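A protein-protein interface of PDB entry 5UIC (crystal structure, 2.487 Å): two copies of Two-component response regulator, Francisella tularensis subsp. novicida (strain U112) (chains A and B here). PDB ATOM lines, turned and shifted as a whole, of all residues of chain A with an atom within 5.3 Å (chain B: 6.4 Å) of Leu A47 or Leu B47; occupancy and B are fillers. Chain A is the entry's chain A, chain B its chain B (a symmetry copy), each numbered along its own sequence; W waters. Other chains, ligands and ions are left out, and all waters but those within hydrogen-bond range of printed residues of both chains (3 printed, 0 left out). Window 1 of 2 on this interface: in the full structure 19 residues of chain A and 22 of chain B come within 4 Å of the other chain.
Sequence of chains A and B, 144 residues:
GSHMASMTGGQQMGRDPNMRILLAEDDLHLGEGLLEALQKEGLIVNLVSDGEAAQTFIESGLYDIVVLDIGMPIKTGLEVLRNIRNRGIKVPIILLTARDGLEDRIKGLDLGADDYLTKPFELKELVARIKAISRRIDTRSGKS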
ATOM      1  N   LEU A  22       0.896 -28.349  -9.319  1.00  0.00           N
ATOM      2  CA  LEU A  22       1.996 -27.627  -9.943  1.00  0.00           C
ATOM      3  C   LEU A  22       2.234 -26.321  -9.197  1.00  0.00           C
ATOM      4  O   LEU A  22       1.303 -25.532  -9.006  1.00  0.00           O
ATOM      5  CB  LEU A  22       1.699 -27.338 -11.416  1.00  0.00           C
ATOM      6  CG  LEU A  22       2.708 -26.444 -12.145  1.00  0.00           C
ATOM      7  CD1 LEU A  22       4.076 -27.111 -12.199  1.00  0.00           C
ATOM      8  CD2 LEU A  22       2.219 -26.108 -13.544  1.00  0.00           C
ATOM      9  N   LEU A  23       3.476 -26.102  -8.776  1.00  0.00           N
ATOM     10  CA  LEU A  23       3.903 -24.838  -8.188  1.00  0.00           C
ATOM     11  C   LEU A  23       4.793 -24.121  -9.193  1.00  0.00           C
ATOM     12  O   LEU A  23       5.832 -24.655  -9.597  1.00  0.00           O
ATOM     13  CB  LEU A  23       4.652 -25.062  -6.874  1.00  0.00           C
ATOM     14  CG  LEU A  23       3.919 -25.856  -5.793  1.00  0.00           C
ATOM     15  CD1 LEU A  23       4.794 -25.974  -4.554  1.00  0.00           C
ATOM     16  CD2 LEU A  23       2.582 -25.211  -5.448  1.00  0.00           C
ATOM     17  N   ALA A  24       4.387 -22.920  -9.596  1.00  0.00           N
ATOM     18  CA  ALA A  24       5.140 -22.099 -10.540  1.00  0.00           C
ATOM     19  C   ALA A  24       5.577 -20.836  -9.801  1.00  0.00           C
ATOM     20  O   ALA A  24       4.868 -19.828  -9.806  1.00  0.00           O
ATOM     21  CB  ALA A  24       4.298 -21.772 -11.771  1.00  0.00           C
ATOM     22  N   GLU A  25       6.747 -20.897  -9.165  1.00  0.00           N
ATOM     23  CA  GLU A  25       7.250 -19.798  -8.347  1.00  0.00           C
ATOM     24  C   GLU A  25       8.738 -19.636  -8.613  1.00  0.00           C
ATOM     25  O   GLU A  25       9.505 -20.586  -8.441  1.00  0.00           O
ATOM     26  CB  GLU A  25       6.994 -20.064  -6.858  1.00  0.00           C
ATOM     27  CG  GLU A  25       7.602 -19.044  -5.906  1.00  0.00           C
ATOM     28  CD  GLU A  25       7.020 -17.653  -6.083  1.00  0.00           C
ATOM     29  OE1 GLU A  25       5.791 -17.497  -5.920  1.00  0.00           O
ATOM     30  OE2 GLU A  25       7.790 -16.716  -6.386  1.00  0.00           O
ATOM     31  N   GLY A  31       9.245 -21.632  -2.905  1.00  0.00           N
ATOM     32  CA  GLY A  31       9.044 -22.901  -3.584  1.00  0.00           C
ATOM     33  C   GLY A  31       9.304 -24.092  -2.682  1.00  0.00           C
ATOM     34  O   GLY A  31       8.476 -25.000  -2.577  1.00  0.00           O
ATOM     35  N   GLU A  32      10.460 -24.104  -2.016  1.00  0.00           N
ATOM     36  CA  GLU A  32      10.807 -25.245  -1.173  1.00  0.00           C
ATOM     37  C   GLU A  32       9.904 -25.323   0.052  1.00  0.00           C
ATOM     38  O   GLU A  32       9.530 -26.420   0.481  1.00  0.00           O
ATOM     39  CB  GLU A  32      12.275 -25.163  -0.755  1.00  0.00           C
ATOM     40  CG  GLU A  32      12.775 -26.400  -0.021  1.00  0.00           C
ATOM     41  CD  GLU A  32      14.291 -26.497   0.008  1.00  0.00           C
ATOM     42  OE1 GLU A  32      14.961 -25.548  -0.450  1.00  0.00           O
ATOM     43  OE2 GLU A  32      14.811 -27.527   0.488  1.00  0.00           O
ATOM     44  N   LEU A  35       6.716 -26.733  -1.058  1.00  0.00           N
ATOM     45  CA  LEU A  35       7.019 -28.124  -1.369  1.00  0.00           C
ATOM     46  C   LEU A  35       6.969 -28.985  -0.113  1.00  0.00           C
ATOM     47  O   LEU A  35       6.276 -30.007  -0.068  1.00  0.00           O
ATOM     48  CB  LEU A  35       8.396 -28.197  -2.027  1.00  0.00           C
ATOM     49  CG  LEU A  35       8.755 -29.370  -2.932  1.00  0.00           C
ATOM     50  CD1 LEU A  35       7.767 -29.522  -4.078  1.00  0.00           C
ATOM     51  CD2 LEU A  35      10.159 -29.133  -3.461  1.00  0.00           C
ATOM     52  N   VAL A  45       3.502 -32.946  -5.628  1.00  0.00           N
ATOM     53  CA  VAL A  45       3.774 -31.545  -5.936  1.00  0.00           C
ATOM     54  C   VAL A  45       4.985 -31.458  -6.855  1.00  0.00           C
ATOM     55  O   VAL A  45       6.025 -32.065  -6.584  1.00  0.00           O
ATOM     56  CB  VAL A  45       4.016 -30.722  -4.655  1.00  0.00           C
ATOM     57  CG1 VAL A  45       3.938 -29.230  -4.957  1.00  0.00           C
ATOM     58  CG2 VAL A  45       3.018 -31.109  -3.574  1.00  0.00           C
ATOM     59  N   ASN A  46       4.850 -30.694  -7.935  1.00  0.00           N
ATOM     60  CA  ASN A  46       5.939 -30.401  -8.851  1.00  0.00           C
ATOM     61  C   ASN A  46       6.218 -28.903  -8.831  1.00  0.00           C
ATOM     62  O   ASN A  46       5.358 -28.099  -8.465  1.00  0.00           O
ATOM     63  CB  ASN A  46       5.606 -30.865 -10.274  1.00  0.00           C
ATOM     64  CG  ASN A  46       5.339 -32.358 -10.351  1.00  0.00           C
ATOM     65  OD1 ASN A  46       5.697 -33.112  -9.447  1.00  0.00           O
ATOM     66  ND2 ASN A  46       4.711 -32.793 -11.437  1.00  0.00           N
ATOM     67  N   LEU A  47       7.431 -28.529  -9.234  1.00  0.00           N
ATOM     68  CA  LEU A  47       7.893 -27.151  -9.121  1.00  0.00           C
ATOM     69  C   LEU A  47       8.537 -26.705 -10.425  1.00  0.00           C
ATOM     70  O   LEU A  47       9.467 -27.351 -10.916  1.00  0.00           O
ATOM     71  CB  LEU A  47       8.881 -27.002  -7.958  1.00  0.00           C
ATOM     72  CG  LEU A  47       9.561 -25.637  -7.805  1.00  0.00           C
ATOM     73  CD1 LEU A  47       8.535 -24.534  -7.607  1.00  0.00           C
ATOM     74  CD2 LEU A  47      10.548 -25.658  -6.648  1.00  0.00           C
ATOM     75  N   VAL A  48       8.032 -25.604 -10.982  1.00  0.00           N
ATOM     76  CA  VAL A  48       8.687 -24.879 -12.059  1.00  0.00           C
ATOM     77  C   VAL A  48       8.850 -23.430 -11.613  1.00  0.00           C
ATOM     78  O   VAL A  48       8.348 -23.020 -10.568  1.00  0.00           O
ATOM     79  CB  VAL A  48       7.911 -24.959 -13.389  1.00  0.00           C
ATOM     80  CG1 VAL A  48       7.740 -26.409 -13.817  1.00  0.00           C
ATOM     81  CG2 VAL A  48       6.562 -24.264 -13.270  1.00  0.00           C
ATOM     82  N   SER A  49       9.558 -22.646 -12.431  1.00  0.00           N
ATOM     83  CA  SER A  49       9.942 -21.304 -12.013  1.00  0.00           C
ATOM     84  C   SER A  49       9.898 -20.274 -13.138  1.00  0.00           C
ATOM     85  O   SER A  49      10.416 -19.166 -12.955  1.00  0.00           O
ATOM     86  CB  SER A  49      11.344 -21.331 -11.393  1.00  0.00           C
ATOM     87  OG  SER A  49      12.266 -21.986 -12.244  1.00  0.00           O
ATOM     88  N   ILE B  21      17.451 -27.512 -15.641  1.00  0.00           N
ATOM     89  CA  ILE B  21      17.672 -28.927 -15.384  1.00  0.00           C
ATOM     90  C   ILE B  21      16.434 -29.499 -14.706  1.00  0.00           C
ATOM     91  O   ILE B  21      15.802 -28.834 -13.879  1.00  0.00           O
ATOM     92  CB  ILE B  21      18.931 -29.168 -14.521  1.00  0.00           C
ATOM     93  CG1 ILE B  21      18.793 -28.500 -13.151  1.00  0.00           C
ATOM     94  CG2 ILE B  21      20.167 -28.637 -15.238  1.00  0.00           C
ATOM     95  CD1 ILE B  21      19.890 -28.874 -12.182  1.00  0.00           C
ATOM     96  N   LEU B  22      16.093 -30.733 -15.060  1.00  0.00           N
ATOM     97  CA  LEU B  22      14.959 -31.433 -14.481  1.00  0.00           C
ATOM     98  C   LEU B  22      15.460 -32.478 -13.493  1.00  0.00           C
ATOM     99  O   LEU B  22      16.411 -33.210 -13.789  1.00  0.00           O
ATOM    100  CB  LEU B  22      14.122 -32.101 -15.572  1.00  0.00           C
ATOM    101  CG  LEU B  22      12.968 -32.983 -15.097  1.00  0.00           C
ATOM    102  CD1 LEU B  22      11.931 -32.147 -14.364  1.00  0.00           C
ATOM    103  CD2 LEU B  22      12.338 -33.724 -16.269  1.00  0.00           C
ATOM    104  N   LEU B  23      14.829 -32.540 -12.323  1.00  0.00           N
ATOM    105  CA  LEU B  23      15.086 -33.595 -11.348  1.00  0.00           C
ATOM    106  C   LEU B  23      13.790 -34.361 -11.133  1.00  0.00           C
ATOM    107  O   LEU B  23      12.835 -33.825 -10.562  1.00  0.00           O
ATOM    108  CB  LEU B  23      15.611 -33.033 -10.030  1.00  0.00           C
ATOM    109  CG  LEU B  23      16.951 -32.307 -10.127  1.00  0.00           C
ATOM    110  CD1 LEU B  23      16.726 -30.808 -10.209  1.00  0.00           C
ATOM    111  CD2 LEU B  23      17.852 -32.662  -8.950  1.00  0.00           C
ATOM    112  N   ALA B  24      13.763 -35.604 -11.597  1.00  0.00           N
ATOM    113  CA  ALA B  24      12.625 -36.498 -11.427  1.00  0.00           C
ATOM    114  C   ALA B  24      13.023 -37.550 -10.401  1.00  0.00           C
ATOM    115  O   ALA B  24      13.865 -38.409 -10.682  1.00  0.00           O
ATOM    116  CB  ALA B  24      12.235 -37.137 -12.759  1.00  0.00           C
ATOM    117  N   LEU B  28      12.152 -36.706  -2.591  1.00  0.00           N
ATOM    118  CA  LEU B  28      12.519 -35.300  -2.684  1.00  0.00           C
ATOM    119  C   LEU B  28      13.291 -34.896  -1.435  1.00  0.00           C
ATOM    120  O   LEU B  28      12.849 -35.155  -0.312  1.00  0.00           O
ATOM    121  CB  LEU B  28      11.278 -34.427  -2.854  1.00  0.00           C
ATOM    122  CG  LEU B  28      11.508 -33.117  -3.610  1.00  0.00           C
ATOM    123  CD1 LEU B  28      10.212 -32.646  -4.245  1.00  0.00           C
ATOM    124  CD2 LEU B  28      12.081 -32.044  -2.692  1.00  0.00           C
ATOM    125  N   LEU B  35      18.175 -26.550  -4.000  1.00  0.00           N
ATOM    126  CA  LEU B  35      17.751 -25.563  -4.987  1.00  0.00           C
ATOM    127  C   LEU B  35      18.713 -24.381  -5.033  1.00  0.00           C
ATOM    128  O   LEU B  35      19.180 -23.988  -6.110  1.00  0.00           O
ATOM    129  CB  LEU B  35      16.330 -25.086  -4.682  1.00  0.00           C
ATOM    130  CG  LEU B  35      15.205 -26.126  -4.729  1.00  0.00           C
ATOM    131  CD1 LEU B  35      13.857 -25.425  -4.864  1.00  0.00           C
ATOM    132  CD2 LEU B  35      15.400 -27.130  -5.858  1.00  0.00           C
ATOM    133  N   VAL B  45      16.325 -25.125 -11.500  1.00  0.00           N
ATOM    134  CA  VAL B  45      15.821 -26.468 -11.217  1.00  0.00           C
ATOM    135  C   VAL B  45      14.308 -26.520 -11.390  1.00  0.00           C
ATOM    136  O   VAL B  45      13.593 -25.560 -11.070  1.00  0.00           O
ATOM    137  CB  VAL B  45      16.222 -26.904  -9.793  1.00  0.00           C
ATOM    138  CG1 VAL B  45      15.255 -27.965  -9.246  1.00  0.00           C
ATOM    139  CG2 VAL B  45      17.645 -27.432  -9.783  1.00  0.00           C
ATOM    140  N   ASN B  46      13.824 -27.656 -11.890  1.00  0.00           N
ATOM    141  CA  ASN B  46      12.412 -28.005 -11.890  1.00  0.00           C
ATOM    142  C   ASN B  46      12.265 -29.420 -11.346  1.00  0.00           C
ATOM    143  O   ASN B  46      13.117 -30.279 -11.586  1.00  0.00           O
ATOM    144  CB  ASN B  46      11.807 -27.907 -13.299  1.00  0.00           C
ATOM    145  CG  ASN B  46      11.691 -26.476 -13.784  1.00  0.00           C
ATOM    146  OD1 ASN B  46      12.085 -25.539 -13.092  1.00  0.00           O
ATOM    147  ND2 ASN B  46      11.150 -26.300 -14.985  1.00  0.00           N
ATOM    148  N   LEU B  47      11.178 -29.661 -10.613  1.00  0.00           N
ATOM    149  CA  LEU B  47      11.009 -30.892  -9.848  1.00  0.00           C
ATOM    150  C   LEU B  47       9.745 -31.635 -10.259  1.00  0.00           C
ATOM    151  O   LEU B  47       8.682 -31.029 -10.433  1.00  0.00           O
ATOM    152  CB  LEU B  47      10.947 -30.595  -8.348  1.00  0.00           C
ATOM    153  CG  LEU B  47      12.151 -29.867  -7.751  1.00  0.00           C
ATOM    154  CD1 LEU B  47      11.891 -29.529  -6.294  1.00  0.00           C
ATOM    155  CD2 LEU B  47      13.414 -30.702  -7.890  1.00  0.00           C
ATOM    156  N   VAL B  48       9.872 -32.954 -10.408  1.00  0.00           N
ATOM    157  CA  VAL B  48       8.741 -33.860 -10.569  1.00  0.00           C
ATOM    158  C   VAL B  48       9.052 -35.136  -9.795  1.00  0.00           C
ATOM    159  O   VAL B  48      10.186 -35.369  -9.372  1.00  0.00           O
ATOM    160  CB  VAL B  48       8.439 -34.185 -12.051  1.00  0.00           C
ATOM    161  CG1 VAL B  48       7.996 -32.935 -12.793  1.00  0.00           C
ATOM    162  CG2 VAL B  48       9.654 -34.811 -12.722  1.00  0.00           C
ATOM    163  N   SER B  49       8.025 -35.972  -9.614  1.00  0.00           N
ATOM    164  CA  SER B  49       8.165 -37.155  -8.775  1.00  0.00           C
ATOM    165  C   SER B  49       7.487 -38.398  -9.344  1.00  0.00           C
ATOM    166  O   SER B  49       7.336 -39.387  -8.616  1.00  0.00           O
ATOM    167  CB  SER B  49       7.612 -36.868  -7.375  1.00  0.00           C
ATOM    168  OG  SER B  49       6.310 -36.313  -7.445  1.00  0.00           O
ATOM    169  N   PHE B  57       7.646 -33.632 -19.274  1.00  0.00           N
ATOM    170  CA  PHE B  57       8.581 -32.523 -19.130  1.00  0.00           C
ATOM    171  C   PHE B  57       9.747 -32.666 -20.100  1.00  0.00           C
ATOM    172  O   PHE B  57      10.116 -31.713 -20.796  1.00  0.00           O
ATOM    173  CB  PHE B  57       9.087 -32.455 -17.689  1.00  0.00           C
ATOM    174  CG  PHE B  57       8.155 -31.749 -16.743  1.00  0.00           C
ATOM    175  CD1 PHE B  57       6.817 -32.105 -16.661  1.00  0.00           C
ATOM    176  CD2 PHE B  57       8.625 -30.737 -15.921  1.00  0.00           C
ATOM    177  CE1 PHE B  57       5.969 -31.456 -15.786  1.00  0.00           C
ATOM    178  CE2 PHE B  57       7.780 -30.089 -15.038  1.00  0.00           C
ATOM    179  CZ  PHE B  57       6.454 -30.447 -14.973  1.00  0.00           C
ATOM    180  N   TYR B  63      14.570 -28.517 -21.334  1.00  0.00           N
ATOM    181  CA  TYR B  63      15.626 -28.826 -20.386  1.00  0.00           C
ATOM    182  C   TYR B  63      16.921 -29.159 -21.111  1.00  0.00           C
ATOM    183  O   TYR B  63      16.910 -29.788 -22.173  1.00  0.00           O
ATOM    184  CB  TYR B  63      15.207 -29.985 -19.482  1.00  0.00           C
ATOM    185  CG  TYR B  63      14.020 -29.623 -18.631  1.00  0.00           C
ATOM    186  CD1 TYR B  63      12.735 -30.000 -18.996  1.00  0.00           C
ATOM    187  CD2 TYR B  63      14.180 -28.866 -17.482  1.00  0.00           C
ATOM    188  CE1 TYR B  63      11.649 -29.650 -18.225  1.00  0.00           C
ATOM    189  CE2 TYR B  63      13.103 -28.512 -16.707  1.00  0.00           C
ATOM    190  CZ  TYR B  63      11.839 -28.908 -17.079  1.00  0.00           C
ATOM    191  OH  TYR B  63      10.759 -28.550 -16.307  1.00  0.00           O
HETATM  192  O   HOH W   1      11.175 -23.429 -14.750  1.00  0.00           O
HETATM  193  O   HOH W   2       5.925 -34.638  -4.848  1.00  0.00           O
HETATM  194  O   HOH W   3       5.453 -35.558 -10.357  1.00  0.00           O
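Of chain B, only Leu B35, Asn B46 and Leu B47 come within 4 Å of Leu A47. Of the printed residues of chain A, Leu B47 touches Leu A35, Asn A46 and Leu A47. Printed residues of chain B within 4 Å of Val A48: Asn B46 and Phe B57. Printed residues of chain B within 4 Å of Asn A46: Leu B47, Val B48 and Ser B49. The nearest residue of chain B that does not touch Leu A47 is Val B45 (4.5 Å). The nearest residue of chain A that does not touch Leu B47 is Val A45 (4.8 Å).
Water W3 lies within hydrogen-bond range of OD1 of Asn A46 (2.6 Å) and N of Ser B49 (2.7 Å). Water W1 lies within hydrogen-bond range of the side-chain amide oxygen (OD1) of Asn B46 (2.8 Å) and the backbone NH (N) of Ser A49 (2.9 Å). Water W2 bridges N of Val A45 (3.1 Å) and OG of Ser B49 (3.1 Å).
Of the 13 printed residues of chain B, 8 touch a printed residue of chain A. Hydrophobic or aromatic side chains of chain B within 4 Å of the printed part of chain A: Leu B28, Leu B35, Leu B47, Val B48 and Phe B57. Of the 12 printed residues of chain A, 5 touch a printed residue of chain B. Hydrophobic or aromatic side chains of chain A within 4 Å of the printed part of chain B: Leu A35, Leu A47 and Val A48. Along chain A the printed residues that touch a printed residue of chain B span positions 35 to 49. Among the printed residues, 12 pairs touch across the chains.
Leu A35 touches Leu B47 (CD2 to CD1, 3.3 Å). CB of Asn A46 touches O of Leu B47, at 3.1 Å. Asn A46 touches Val B48 (OD1 to CA, 3.3 Å). Asn A46 touches Ser B49 (OD1 to N, 3.7 Å). Leu A47 touches Leu B35 (CD2 to CD1, 3.8 Å). Leu A47 touches Asn B46 (O to CA, 3.2 Å). CG1 of Val A48 touches ND2 of Asn B46 (3.6 Å). CE2 of Phe B57 touches CG1 of Val A48 (3.9 Å). Ser A49 touches Val B45 (OG to O, 3.99 Å). OD1 of Asn B46 touches OG of Ser A49 (3.7 Å).
O of Asn A46 lies within hydrogen-bond range of N of Leu A23, at 2.8 Å. The backbone carbonyl oxygen of Leu B23 sits at hydrogen-bond distance from the backbone NH of Val B48, at 3.1 Å. The backbone NH (N) of Glu A25 is in hydrogen-bond range of the backbone carbonyl oxygen (O) of Val A48. The backbone carbonyl oxygen (O) of Leu A23 is in hydrogen-bond range of the backbone NH (N) of Val A48, at 2.8 Å. The backbone carbonyl oxygen (O) of Ile B21 lies within hydrogen-bond range of the backbone NH (N) of Asn B46 (3.0 Å). The side-chain amide nitrogen of Asn B46 is in hydrogen-bond range of the side-chain hydroxyl of Tyr B63 (2.6 Å).
Asn A46 touches Leu B47, and with the chains exchanged Leu A47 touches Asn B46. Asn A46 touches Val B48, and with the chains exchanged Val A48 touches Asn B46. Asn A46 touches Ser B49, and with the chains exchanged Ser A49 touches Asn B46. Ser A49 touches Val B45, but with the chains exchanged Val A45 does not touch Ser B49 (4.3 Å). 9 positions are printed for both chains. Of the 12 pairs that touch across the chains among the printed residues, 9 have their exchanged pair printed and touching as well.
O of Leu A47 lies within hydrogen-bond range of N of Leu B47 (2.9 Å).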
